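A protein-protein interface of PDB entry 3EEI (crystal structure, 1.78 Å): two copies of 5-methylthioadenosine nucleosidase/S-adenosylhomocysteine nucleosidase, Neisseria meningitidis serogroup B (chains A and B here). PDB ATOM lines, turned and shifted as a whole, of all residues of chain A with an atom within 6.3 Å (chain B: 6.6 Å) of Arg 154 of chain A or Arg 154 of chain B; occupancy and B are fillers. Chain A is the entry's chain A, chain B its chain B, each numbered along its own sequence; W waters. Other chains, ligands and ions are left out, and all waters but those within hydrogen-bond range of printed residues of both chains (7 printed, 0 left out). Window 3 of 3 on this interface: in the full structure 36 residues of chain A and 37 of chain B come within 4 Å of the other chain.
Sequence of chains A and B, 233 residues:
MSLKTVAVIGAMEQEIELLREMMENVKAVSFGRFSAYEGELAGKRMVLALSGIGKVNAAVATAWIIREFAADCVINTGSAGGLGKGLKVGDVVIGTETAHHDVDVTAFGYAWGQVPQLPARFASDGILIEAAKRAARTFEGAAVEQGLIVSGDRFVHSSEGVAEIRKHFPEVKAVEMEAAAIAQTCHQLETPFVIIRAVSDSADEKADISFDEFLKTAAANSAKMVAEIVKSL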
ATOM      1  N   HIS A 101      10.729 -23.752   1.650  1.00  0.00           N
ATOM      2  CA  HIS A 101       9.649 -22.975   2.215  1.00  0.00           C
ATOM      3  C   HIS A 101      10.137 -21.618   2.762  1.00  0.00           C
ATOM      4  O   HIS A 101       9.314 -20.714   2.994  1.00  0.00           O
ATOM      5  CB  HIS A 101       8.892 -23.746   3.301  1.00  0.00           C
ATOM      6  CG  HIS A 101       9.674 -23.962   4.555  1.00  0.00           C
ATOM      7  ND1 HIS A 101       9.912 -22.956   5.455  1.00  0.00           N
ATOM      8  CD2 HIS A 101      10.217 -25.082   5.093  1.00  0.00           C
ATOM      9  CE1 HIS A 101      10.596 -23.427   6.487  1.00  0.00           C
ATOM     10  NE2 HIS A 101      10.806 -24.716   6.289  1.00  0.00           N
ATOM     11  N   ASP A 102      11.448 -21.468   2.890  1.00  0.00           N
ATOM     12  CA  ASP A 102      12.025 -20.247   3.453  1.00  0.00           C
ATOM     13  C   ASP A 102      12.791 -19.377   2.485  1.00  0.00           C
ATOM     14  O   ASP A 102      13.433 -18.388   2.908  1.00  0.00           O
ATOM     15  CB  ASP A 102      12.927 -20.543   4.669  1.00  0.00           C
ATOM     16  CG  ASP A 102      14.189 -21.328   4.306  1.00  0.00           C
ATOM     17  OD1 ASP A 102      14.361 -21.829   3.181  1.00  0.00           O
ATOM     18  OD2 ASP A 102      15.016 -21.569   5.208  1.00  0.00           O
ATOM     19  N   VAL A 103      12.704 -19.685   1.199  1.00  0.00           N
ATOM     20  CA  VAL A 103      13.268 -18.766   0.184  1.00  0.00           C
ATOM     21  C   VAL A 103      12.255 -17.652  -0.175  1.00  0.00           C
ATOM     22  O   VAL A 103      11.103 -17.937  -0.451  1.00  0.00           O
ATOM     23  CB  VAL A 103      13.643 -19.541  -1.089  1.00  0.00           C
ATOM     24  CG1 VAL A 103      13.960 -18.539  -2.237  1.00  0.00           C
ATOM     25  CG2 VAL A 103      14.881 -20.428  -0.829  1.00  0.00           C
ATOM     26  N   ASP A 104      12.695 -16.393  -0.169  1.00  0.00           N
ATOM     27  CA  ASP A 104      11.803 -15.289  -0.470  1.00  0.00           C
ATOM     28  C   ASP A 104      12.587 -14.245  -1.211  1.00  0.00           C
ATOM     29  O   ASP A 104      13.261 -13.417  -0.591  1.00  0.00           O
ATOM     30  CB  ASP A 104      11.277 -14.671   0.804  1.00  0.00           C
ATOM     31  CG  ASP A 104      10.569 -13.357   0.566  1.00  0.00           C
ATOM     32  OD1 ASP A 104      10.283 -12.999  -0.619  1.00  0.00           O
ATOM     33  OD2 ASP A 104      10.332 -12.683   1.584  1.00  0.00           O
ATOM     34  N   VAL A 105      12.500 -14.296  -2.543  1.00  0.00           N
ATOM     35  CA  VAL A 105      13.041 -13.213  -3.369  1.00  0.00           C
ATOM     36  C   VAL A 105      11.841 -12.637  -4.132  1.00  0.00           C
ATOM     37  O   VAL A 105      11.908 -12.295  -5.308  1.00  0.00           O
ATOM     38  CB  VAL A 105      14.128 -13.713  -4.314  1.00  0.00           C
ATOM     39  CG1 VAL A 105      14.872 -12.502  -4.904  1.00  0.00           C
ATOM     40  CG2 VAL A 105      15.125 -14.605  -3.524  1.00  0.00           C
ATOM     41  N   GLY A 152      13.520 -26.038   4.786  1.00  0.00           N
ATOM     42  CA  GLY A 152      14.173 -24.800   5.094  1.00  0.00           C
ATOM     43  C   GLY A 152      15.147 -24.966   6.247  1.00  0.00           C
ATOM     44  O   GLY A 152      15.285 -26.056   6.801  1.00  0.00           O
ATOM     45  N   ASP A 153      15.844 -23.885   6.588  1.00  0.00           N
ATOM     46  CA  ASP A 153      16.996 -24.003   7.495  1.00  0.00           C
ATOM     47  C   ASP A 153      16.536 -23.822   8.937  1.00  0.00           C
ATOM     48  O   ASP A 153      17.211 -23.214   9.776  1.00  0.00           O
ATOM     49  CB  ASP A 153      18.137 -23.063   7.097  1.00  0.00           C
ATOM     50  CG  ASP A 153      19.319 -23.795   6.506  1.00  0.00           C
ATOM     51  OD1 ASP A 153      20.261 -23.118   6.049  1.00  0.00           O
ATOM     52  OD2 ASP A 153      19.321 -25.051   6.526  1.00  0.00           O
ATOM     53  N   ARG A 154      15.378 -24.385   9.229  1.00  0.00           N
ATOM     54  CA  ARG A 154      14.867 -24.304  10.582  1.00  0.00           C
ATOM     55  C   ARG A 154      14.140 -25.564  10.990  1.00  0.00           C
ATOM     56  O   ARG A 154      13.513 -26.234  10.162  1.00  0.00           O
ATOM     57  CB  ARG A 154      13.912 -23.110  10.718  1.00  0.00           C
ATOM     58  CG  ARG A 154      12.578 -23.292  10.040  1.00  0.00           C
ATOM     59  CD  ARG A 154      11.744 -21.971  10.104  1.00  0.00           C
ATOM     60  NE  ARG A 154      12.311 -20.977   9.194  1.00  0.00           N
ATOM     61  CZ  ARG A 154      11.681 -19.870   8.824  1.00  0.00           C
ATOM     62  NH1 ARG A 154      12.275 -18.985   8.019  1.00  0.00           N
ATOM     63  NH2 ARG A 154      10.447 -19.634   9.279  1.00  0.00           N
ATOM     64  N   PHE A 155      14.211 -25.881  12.288  1.00  0.00           N
ATOM     65  CA  PHE A 155      13.430 -26.978  12.802  1.00  0.00           C
ATOM     66  C   PHE A 155      12.108 -26.375  13.224  1.00  0.00           C
ATOM     67  O   PHE A 155      12.070 -25.489  14.095  1.00  0.00           O
ATOM     68  CB  PHE A 155      14.111 -27.577  14.045  1.00  0.00           C
ATOM     69  CG  PHE A 155      13.366 -28.718  14.591  1.00  0.00           C
ATOM     70  CD1 PHE A 155      13.505 -29.971  14.005  1.00  0.00           C
ATOM     71  CD2 PHE A 155      12.504 -28.552  15.672  1.00  0.00           C
ATOM     72  CE1 PHE A 155      12.817 -31.066  14.490  1.00  0.00           C
ATOM     73  CE2 PHE A 155      11.789 -29.648  16.172  1.00  0.00           C
ATOM     74  CZ  PHE A 155      11.959 -30.903  15.591  1.00  0.00           C
ATOM     75  N   VAL A 156      11.029 -26.815  12.588  1.00  0.00           N
ATOM     76  CA  VAL A 156       9.727 -26.214  12.831  1.00  0.00           C
ATOM     77  C   VAL A 156       9.039 -26.873  14.015  1.00  0.00           C
ATOM     78  O   VAL A 156       8.890 -28.084  14.016  1.00  0.00           O
ATOM     79  CB  VAL A 156       8.839 -26.398  11.603  1.00  0.00           C
ATOM     80  CG1 VAL A 156       7.460 -25.744  11.835  1.00  0.00           C
ATOM     81  CG2 VAL A 156       9.493 -25.717  10.376  1.00  0.00           C
ATOM     82  N   GLY A 161       4.296 -21.613  12.997  1.00  0.00           N
ATOM     83  CA  GLY A 161       5.322 -21.947  11.992  1.00  0.00           C
ATOM     84  C   GLY A 161       4.706 -22.828  10.920  1.00  0.00           C
ATOM     85  O   GLY A 161       4.936 -22.628   9.731  1.00  0.00           O
ATOM     86  N   GLU A 164       2.371 -20.790   8.632  1.00  0.00           N
ATOM     87  CA  GLU A 164       3.083 -20.013   7.606  1.00  0.00           C
ATOM     88  C   GLU A 164       3.391 -20.852   6.390  1.00  0.00           C
ATOM     89  O   GLU A 164       3.268 -20.406   5.245  1.00  0.00           O
ATOM     90  CB  GLU A 164       4.400 -19.494   8.150  1.00  0.00           C
ATOM     91  CG  GLU A 164       4.225 -18.301   9.029  1.00  0.00           C
ATOM     92  CD  GLU A 164       5.539 -17.689   9.532  1.00  0.00           C
ATOM     93  OE1 GLU A 164       6.560 -18.400   9.675  1.00  0.00           O
ATOM     94  OE2 GLU A 164       5.517 -16.476   9.828  1.00  0.00           O
ATOM     95  N   ILE A 165       3.840 -22.062   6.635  1.00  0.00           N
ATOM     96  CA  ILE A 165       4.244 -22.910   5.531  1.00  0.00           C
ATOM     97  C   ILE A 165       3.003 -23.336   4.739  1.00  0.00           C
ATOM     98  O   ILE A 165       2.977 -23.295   3.490  1.00  0.00           O
ATOM     99  CB  ILE A 165       4.937 -24.163   6.101  1.00  0.00           C
ATOM    100  CG1 ILE A 165       6.329 -23.808   6.651  1.00  0.00           C
ATOM    101  CG2 ILE A 165       4.915 -25.308   5.030  1.00  0.00           C
ATOM    102  CD1 ILE A 165       7.057 -24.951   7.426  1.00  0.00           C
ATOM    103  N   VAL A 175       7.722 -31.558   6.194  1.00  0.00           N
ATOM    104  CA  VAL A 175       8.710 -30.486   6.270  1.00  0.00           C
ATOM    105  C   VAL A 175       9.977 -30.996   6.911  1.00  0.00           C
ATOM    106  O   VAL A 175       9.933 -31.771   7.897  1.00  0.00           O
ATOM    107  CB  VAL A 175       8.194 -29.231   7.038  1.00  0.00           C
ATOM    108  CG1 VAL A 175       7.698 -29.550   8.437  1.00  0.00           C
ATOM    109  CG2 VAL A 175       9.263 -28.138   7.064  1.00  0.00           C
ATOM    110  N   GLU A 176      11.108 -30.588   6.345  1.00  0.00           N
ATOM    111  CA  GLU A 176      12.407 -30.928   6.922  1.00  0.00           C
ATOM    112  C   GLU A 176      13.445 -29.914   6.461  1.00  0.00           C
ATOM    113  O   GLU A 176      13.074 -28.779   6.198  1.00  0.00           O
ATOM    114  CB  GLU A 176      12.778 -32.391   6.692  1.00  0.00           C
ATOM    115  CG  GLU A 176      12.487 -32.912   5.273  1.00  0.00           C
ATOM    116  CD  GLU A 176      13.313 -32.135   4.287  1.00  0.00           C
ATOM    117  OE1 GLU A 176      12.786 -31.134   3.741  1.00  0.00           O
ATOM    118  OE2 GLU A 176      14.506 -32.483   4.103  1.00  0.00           O
ATOM    119  N   MET A 177      14.732 -30.260   6.454  1.00  0.00           N
ATOM    120  CA  MET A 177      15.764 -29.211   6.341  1.00  0.00           C
ATOM    121  C   MET A 177      16.795 -29.489   5.249  1.00  0.00           C
ATOM    122  O   MET A 177      17.729 -28.690   5.092  1.00  0.00           O
ATOM    123  CB  MET A 177      16.506 -29.059   7.685  1.00  0.00           C
ATOM    124  CG  MET A 177      15.570 -28.656   8.789  1.00  0.00           C
ATOM    125  SD  MET A 177      16.345 -28.504  10.444  1.00  0.00           S
ATOM    126  CE  MET A 177      17.697 -27.415  10.151  1.00  0.00           C
ATOM    127  N   LYS B  55      21.858 -19.781  -0.883  1.00  0.00           N
ATOM    128  CA  LYS B  55      22.821 -20.574  -0.109  1.00  0.00           C
ATOM    129  C   LYS B  55      23.242 -21.838  -0.813  1.00  0.00           C
ATOM    130  O   LYS B  55      24.413 -22.205  -0.778  1.00  0.00           O
ATOM    131  CB  LYS B  55      22.225 -20.992   1.217  1.00  0.00           C
ATOM    132  CG  LYS B  55      21.780 -19.856   2.108  1.00  0.00           C
ATOM    133  CD  LYS B  55      21.385 -20.586   3.476  1.00  0.00           C
ATOM    134  CE  LYS B  55      20.549 -19.804   4.334  1.00  0.00           C
ATOM    135  NZ  LYS B  55      20.626 -20.412   5.683  1.00  0.00           N
ATOM    136  N   HIS B 101      21.533 -15.702   9.280  1.00  0.00           N
ATOM    137  CA  HIS B 101      20.496 -15.041  10.084  1.00  0.00           C
ATOM    138  C   HIS B 101      19.176 -15.829  10.112  1.00  0.00           C
ATOM    139  O   HIS B 101      18.318 -15.605  10.962  1.00  0.00           O
ATOM    140  CB  HIS B 101      20.291 -13.599   9.619  1.00  0.00           C
ATOM    141  CG  HIS B 101      19.574 -13.465   8.312  1.00  0.00           C
ATOM    142  ND1 HIS B 101      18.221 -13.698   8.181  1.00  0.00           N
ATOM    143  CD2 HIS B 101      20.003 -13.035   7.102  1.00  0.00           C
ATOM    144  CE1 HIS B 101      17.861 -13.450   6.932  1.00  0.00           C
ATOM    145  NE2 HIS B 101      18.921 -13.052   6.255  1.00  0.00           N
ATOM    146  N   ASP B 102      19.022 -16.782   9.203  1.00  0.00           N
ATOM    147  CA  ASP B 102      17.752 -17.485   9.111  1.00  0.00           C
ATOM    148  C   ASP B 102      17.828 -18.969   9.516  1.00  0.00           C
ATOM    149  O   ASP B 102      16.881 -19.712   9.314  1.00  0.00           O
ATOM    150  CB  ASP B 102      17.198 -17.331   7.666  1.00  0.00           C
ATOM    151  CG  ASP B 102      18.031 -18.058   6.647  1.00  0.00           C
ATOM    152  OD1 ASP B 102      19.142 -18.552   7.019  1.00  0.00           O
ATOM    153  OD2 ASP B 102      17.571 -18.153   5.462  1.00  0.00           O
ATOM    154  N   VAL B 103      18.951 -19.392  10.102  1.00  0.00           N
ATOM    155  CA  VAL B 103      19.046 -20.727  10.660  1.00  0.00           C
ATOM    156  C   VAL B 103      18.466 -20.743  12.063  1.00  0.00           C
ATOM    157  O   VAL B 103      18.849 -19.943  12.896  1.00  0.00           O
ATOM    158  CB  VAL B 103      20.527 -21.240  10.655  1.00  0.00           C
ATOM    159  CG1 VAL B 103      20.703 -22.427  11.546  1.00  0.00           C
ATOM    160  CG2 VAL B 103      20.921 -21.653   9.256  1.00  0.00           C
ATOM    161  N   ASP B 104      17.576 -21.679  12.332  1.00  0.00           N
ATOM    162  CA  ASP B 104      16.958 -21.773  13.669  1.00  0.00           C
ATOM    163  C   ASP B 104      16.740 -23.223  14.059  1.00  0.00           C
ATOM    164  O   ASP B 104      15.769 -23.844  13.650  1.00  0.00           O
ATOM    165  CB  ASP B 104      15.618 -21.069  13.655  1.00  0.00           C
ATOM    166  CG  ASP B 104      14.771 -21.361  14.897  1.00  0.00           C
ATOM    167  OD1 ASP B 104      15.286 -21.962  15.873  1.00  0.00           O
ATOM    168  OD2 ASP B 104      13.576 -20.959  14.855  1.00  0.00           O
ATOM    169  N   VAL B 105      17.675 -23.771  14.825  1.00  0.00           N
ATOM    170  CA  VAL B 105      17.485 -25.074  15.443  1.00  0.00           C
ATOM    171  C   VAL B 105      17.532 -24.842  16.977  1.00  0.00           C
ATOM    172  O   VAL B 105      18.059 -25.657  17.738  1.00  0.00           O
ATOM    173  CB  VAL B 105      18.555 -26.093  14.976  1.00  0.00           C
ATOM    174  CG1 VAL B 105      18.171 -27.522  15.374  1.00  0.00           C
ATOM    175  CG2 VAL B 105      18.695 -26.055  13.457  1.00  0.00           C
ATOM    176  N   TRP B 112      20.777 -19.016  18.082  1.00  0.00           N
ATOM    177  CA  TRP B 112      20.177 -18.529  16.828  1.00  0.00           C
ATOM    178  C   TRP B 112      21.242 -18.444  15.735  1.00  0.00           C
ATOM    179  O   TRP B 112      22.304 -17.878  15.973  1.00  0.00           O
ATOM    180  CB  TRP B 112      19.562 -17.137  17.024  1.00  0.00           C
ATOM    181  CG  TRP B 112      18.795 -16.824  15.814  1.00  0.00           C
ATOM    182  CD1 TRP B 112      19.264 -16.265  14.655  1.00  0.00           C
ATOM    183  CD2 TRP B 112      17.442 -17.187  15.579  1.00  0.00           C
ATOM    184  NE1 TRP B 112      18.248 -16.213  13.719  1.00  0.00           N
ATOM    185  CE2 TRP B 112      17.126 -16.792  14.258  1.00  0.00           C
ATOM    186  CE3 TRP B 112      16.451 -17.799  16.372  1.00  0.00           C
ATOM    187  CZ2 TRP B 112      15.850 -16.948  13.722  1.00  0.00           C
ATOM    188  CZ3 TRP B 112      15.200 -17.990  15.824  1.00  0.00           C
ATOM    189  CH2 TRP B 112      14.905 -17.547  14.514  1.00  0.00           C
ATOM    190  N   SER B 151      23.699 -13.847   6.413  1.00  0.00           N
ATOM    191  CA  SER B 151      23.115 -14.302   5.158  1.00  0.00           C
ATOM    192  C   SER B 151      21.898 -15.190   5.432  1.00  0.00           C
ATOM    193  O   SER B 151      21.797 -15.872   6.442  1.00  0.00           O
ATOM    194  CB  SER B 151      24.096 -15.203   4.395  1.00  0.00           C
ATOM    195  OG  SER B 151      25.390 -14.627   4.314  1.00  0.00           O
ATOM    196  N   GLY B 152      20.998 -15.214   4.469  1.00  0.00           N
ATOM    197  CA  GLY B 152      19.815 -16.009   4.576  1.00  0.00           C
ATOM    198  C   GLY B 152      19.273 -16.133   3.177  1.00  0.00           C
ATOM    199  O   GLY B 152      19.705 -15.420   2.276  1.00  0.00           O
ATOM    200  N   ASP B 153      18.348 -17.059   2.986  1.00  0.00           N
ATOM    201  CA  ASP B 153      17.857 -17.324   1.629  1.00  0.00           C
ATOM    202  C   ASP B 153      16.707 -16.396   1.247  1.00  0.00           C
ATOM    203  O   ASP B 153      15.756 -16.815   0.585  1.00  0.00           O
ATOM    204  CB  ASP B 153      17.421 -18.783   1.471  1.00  0.00           C
ATOM    205  CG  ASP B 153      18.369 -19.581   0.575  1.00  0.00           C
ATOM    206  OD1 ASP B 153      18.237 -20.809   0.523  1.00  0.00           O
ATOM    207  OD2 ASP B 153      19.261 -18.979  -0.072  1.00  0.00           O
ATOM    208  N   ARG B 154      16.815 -15.125   1.623  1.00  0.00           N
ATOM    209  CA  ARG B 154      15.790 -14.177   1.235  1.00  0.00           C
ATOM    210  C   ARG B 154      16.363 -12.784   1.022  1.00  0.00           C
ATOM    211  O   ARG B 154      17.364 -12.416   1.617  1.00  0.00           O
ATOM    212  CB  ARG B 154      14.690 -14.136   2.274  1.00  0.00           C
ATOM    213  CG  ARG B 154      15.099 -13.685   3.661  1.00  0.00           C
ATOM    214  CD  ARG B 154      13.947 -13.972   4.639  1.00  0.00           C
ATOM    215  NE  ARG B 154      14.426 -13.916   6.004  1.00  0.00           N
ATOM    216  CZ  ARG B 154      14.327 -14.890   6.917  1.00  0.00           C
ATOM    217  NH1 ARG B 154      13.708 -16.052   6.669  1.00  0.00           N
ATOM    218  NH2 ARG B 154      14.862 -14.680   8.128  1.00  0.00           N
ATOM    219  N   PHE B 155      15.738 -12.041   0.124  1.00  0.00           N
ATOM    220  CA  PHE B 155      16.065 -10.644  -0.080  1.00  0.00           C
ATOM    221  C   PHE B 155      15.312  -9.799   0.956  1.00  0.00           C
ATOM    222  O   PHE B 155      14.062  -9.795   0.987  1.00  0.00           O
ATOM    223  CB  PHE B 155      15.636 -10.233  -1.472  1.00  0.00           C
ATOM    224  CG  PHE B 155      16.038  -8.842  -1.825  1.00  0.00           C
ATOM    225  CD1 PHE B 155      17.337  -8.567  -2.209  1.00  0.00           C
ATOM    226  CD2 PHE B 155      15.117  -7.811  -1.766  1.00  0.00           C
ATOM    227  CE1 PHE B 155      17.736  -7.287  -2.554  1.00  0.00           C
ATOM    228  CE2 PHE B 155      15.497  -6.490  -2.106  1.00  0.00           C
ATOM    229  CZ  PHE B 155      16.809  -6.234  -2.488  1.00  0.00           C
ATOM    230  N   VAL B 156      16.070  -9.118   1.831  1.00  0.00           N
ATOM    231  CA  VAL B 156      15.487  -8.340   2.910  1.00  0.00           C
ATOM    232  C   VAL B 156      15.089  -6.962   2.425  1.00  0.00           C
ATOM    233  O   VAL B 156      15.936  -6.269   1.881  1.00  0.00           O
ATOM    234  CB  VAL B 156      16.425  -8.285   4.141  1.00  0.00           C
ATOM    235  CG1 VAL B 156      15.709  -7.648   5.315  1.00  0.00           C
ATOM    236  CG2 VAL B 156      16.863  -9.755   4.500  1.00  0.00           C
ATOM    237  N   GLU B 164      14.290  -7.522  13.159  1.00  0.00           N
ATOM    238  CA  GLU B 164      14.507  -8.867  13.688  1.00  0.00           C
ATOM    239  C   GLU B 164      15.939  -9.392  13.519  1.00  0.00           C
ATOM    240  O   GLU B 164      16.465 -10.046  14.417  1.00  0.00           O
ATOM    241  CB  GLU B 164      13.496  -9.883  13.122  1.00  0.00           C
ATOM    242  CG  GLU B 164      14.085 -11.289  12.838  1.00  0.00           C
ATOM    243  CD  GLU B 164      13.269 -12.442  13.436  1.00  0.00           C
ATOM    244  OE1 GLU B 164      13.485 -13.614  13.023  1.00  0.00           O
ATOM    245  OE2 GLU B 164      12.416 -12.171  14.325  1.00  0.00           O
ATOM    246  N   ILE B 165      16.557  -9.111  12.379  1.00  0.00           N
ATOM    247  CA  ILE B 165      17.963  -9.453  12.224  1.00  0.00           C
ATOM    248  C   ILE B 165      18.794  -8.743  13.294  1.00  0.00           C
ATOM    249  O   ILE B 165      19.589  -9.370  13.990  1.00  0.00           O
ATOM    250  CB  ILE B 165      18.476  -9.098  10.824  1.00  0.00           C
ATOM    251  CG1 ILE B 165      17.819 -10.037   9.815  1.00  0.00           C
ATOM    252  CG2 ILE B 165      20.007  -9.197  10.781  1.00  0.00           C
ATOM    253  CD1 ILE B 165      18.059  -9.685   8.343  1.00  0.00           C
ATOM    254  N   VAL B 175      23.804  -7.563   5.167  1.00  0.00           N
ATOM    255  CA  VAL B 175      23.030  -8.803   4.985  1.00  0.00           C
ATOM    256  C   VAL B 175      23.011  -9.146   3.499  1.00  0.00           C
ATOM    257  O   VAL B 175      22.874  -8.267   2.624  1.00  0.00           O
ATOM    258  CB  VAL B 175      21.563  -8.656   5.538  1.00  0.00           C
ATOM    259  CG1 VAL B 175      20.842  -7.405   4.942  1.00  0.00           C
ATOM    260  CG2 VAL B 175      20.714  -9.925   5.262  1.00  0.00           C
ATOM    261  N   GLU B 176      23.159 -10.426   3.173  1.00  0.00           N
ATOM    262  CA  GLU B 176      23.019 -10.814   1.775  1.00  0.00           C
ATOM    263  C   GLU B 176      22.618 -12.281   1.726  1.00  0.00           C
ATOM    264  O   GLU B 176      22.084 -12.760   2.716  1.00  0.00           O
ATOM    265  CB  GLU B 176      24.259 -10.469   0.961  1.00  0.00           C
ATOM    266  CG  GLU B 176      25.551 -10.726   1.649  1.00  0.00           C
ATOM    267  CD  GLU B 176      25.719 -12.168   1.946  1.00  0.00           C
ATOM    268  OE1 GLU B 176      25.411 -12.544   3.100  1.00  0.00           O
ATOM    269  OE2 GLU B 176      26.149 -12.918   1.028  1.00  0.00           O
ATOM    270  N   MET B 177      22.867 -12.993   0.626  1.00  0.00           N
ATOM    271  CA  MET B 177      22.284 -14.347   0.500  1.00  0.00           C
ATOM    272  C   MET B 177      23.281 -15.469   0.274  1.00  0.00           C
ATOM    273  O   MET B 177      22.878 -16.606   0.057  1.00  0.00           O
ATOM    274  CB  MET B 177      21.212 -14.370  -0.580  1.00  0.00           C
ATOM    275  CG  MET B 177      20.022 -13.396  -0.216  1.00  0.00           C
ATOM    276  SD  MET B 177      18.925 -13.274  -1.651  1.00  0.00           S
ATOM    277  CE  MET B 177      18.351 -14.964  -1.820  1.00  0.00           C
HETATM  278  O   HOH W   1      14.744 -20.336   7.577  1.00  0.00           O
HETATM  279  O   HOH W   2      13.998 -24.532  16.298  1.00  0.00           O
HETATM  280  O   HOH W   3      12.553 -11.139   2.751  1.00  0.00           O
HETATM  281  O   HOH W   4      11.699 -22.802  13.493  1.00  0.00           O
HETATM  282  O   HOH W   5      11.945 -10.584  -1.176  1.00  0.00           O
HETATM  283  O   HOH W   6      15.058 -17.410   4.817  1.00  0.00           O
HETATM  284  O   HOH W   7      17.643 -20.696   4.463  1.00  0.00           O
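The backbone NH (N) of Asp 153 of chain A lies within hydrogen-bond range of the side-chain carboxylate (OD2) of Asp 102 of chain A. The side-chain amino group (NZ) of Lys 55 of chain B lies within salt-bridge range of the side-chain carboxylate (OD1) of Asp 102 of chain B. The backbone NH of Lys 55 of chain B lies within hydrogen-bond range of the side-chain carboxylate of Asp 153 of chain B. ND1 of His 101 of chain B sits close to NH2 of Arg 154 of chain B, at 3.5 Å. The side-chain carboxylate (OD2) of Asp 102 of chain B lies within hydrogen-bond range of the backbone NH (N) of Asp 153 of chain B, 2.8 Å away.
Printed residues of chain B within 4 Å of Val 105 of chain A: Met 177. Of chain B, only Asp 104 (3.2 Å) and Arg 154 (3.5 Å) come within 4 Å of Arg 154 of chain A. Ser 151 of chain B touches none of the printed residues of chain A. Of the printed residues of chain A, Asp 153 of chain B touches Asp 102, Val 103 and Asp 104. Arg 154 of chain B touches two residues of chain A. Of the printed residues of chain A, Phe 155 of chain B touches Asp 104. Ile 165 of chain B touches none of the printed residues of chain A. Of the printed residues of chain A, Met 177 of chain B touches Val 105. The nearest residue of chain B that does not touch Arg 154 of chain A is Asp 102 of chain B (4.7 Å). The nearest printed residue of chain A that does not touch Lys 55 of chain B is Asp 102 of chain A (5.7 Å).
The backbone NH of Asp 104 of chain A sits at hydrogen-bond distance from the backbone carbonyl oxygen of Asp 153 of chain B (3.2 Å). O of Asp 104 of chain A is in hydrogen-bond range of N of Phe 155 of chain B, 2.9 Å away. The side-chain amino group (NZ) of Lys 55 of chain B lies within salt-bridge range of the side-chain carboxylate (OD1) of Asp 153 of chain A (2.8 Å). The backbone carbonyl oxygen (O) of Asp 153 of chain A is in hydrogen-bond range of the backbone NH (N) of Asp 104 of chain B, at 3.0 Å. The backbone carbonyl oxygen (O) of Asp 104 of chain B sits at hydrogen-bond distance from the backbone NH (N) of Phe 155 of chain A, at 2.9 Å.
Water W6 lies within hydrogen-bond range of the guanidinium group of Arg 154 of chain B (2.7 Å), the backbone carbonyl oxygen of Asp 102 of chain A (2.7 Å) and the side-chain carboxylate of Asp 102 of chain B (2.7 Å). Water W1 lies within hydrogen-bond range of OD2 of Asp 102 of chain A (2.7 Å), O of Asp 102 of chain B (2.8 Å) and NH1 of Arg 154 of chain A (2.8 Å). Water W4 bridges the backbone carbonyl oxygen of Phe 155 of chain A (2.8 Å) and the side-chain carboxylate of Asp 104 of chain B (3.0 Å). Water W5 bridges the side-chain carboxylate (OD1) of Asp 104 of chain A (3.0 Å) and the backbone carbonyl oxygen (O) of Phe 155 of chain B (3.1 Å).
Val 103 of chain A touches Asp 153 of chain B, and with the chains exchanged Asp 153 of chain A touches Val 103 of chain B. Asp 104 of chain A touches Asp 153 of chain B, and with the chains exchanged Asp 153 of chain A touches Asp 104 of chain B. Val 105 of chain A touches Met 177 of chain B, and with the chains exchanged Met 177 of chain A touches Val 105 of chain B. Arg 154 of chain B touches its own counterpart, Arg 154 of chain A. Of the 14 pairs that touch across the chains among the printed residues, 13 have their exchanged pair printed and touching as well.
Among the printed residues, merely in contact across the chains: Asp 102 of chain A with Asp 153 of chain B, Val 103 of chain A with Asp 153 of chain B, Asp 104 of chain A with Arg 154 of chain B, Val 105 of chain A with Met 177 of chain B, Asp 153 of chain A with Asp 102 of chain B, Asp 153 of chain A with Val 103 of chain B, Arg 154 of chain A with Asp 104 of chain B, Arg 154 of chain A with Arg 154 of chain B and Met 177 of chain A with Val 105 of chain B.
Printed residues of chain B that touch a printed residue of chain A: Lys 55, Asp 102, Val 103, Asp 104, Val 105, Asp 153, Arg 154, Phe 155 and Met 177. Hydrophobic or aromatic side chains of chain B within 4 Å of the printed part of chain A: Val 103, Val 105 and Met 177. Hydrophobic or aromatic side chains of chain A that line the printed part of chain B: Val 103, Val 105 and Met 177. Among the printed residues, Asp or Glu carboxylates within 4 Å of a Lys or Arg side-chain nitrogen of the other chain: Asp 153 of chain A with Lys 55 of chain B (2.8 Å).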
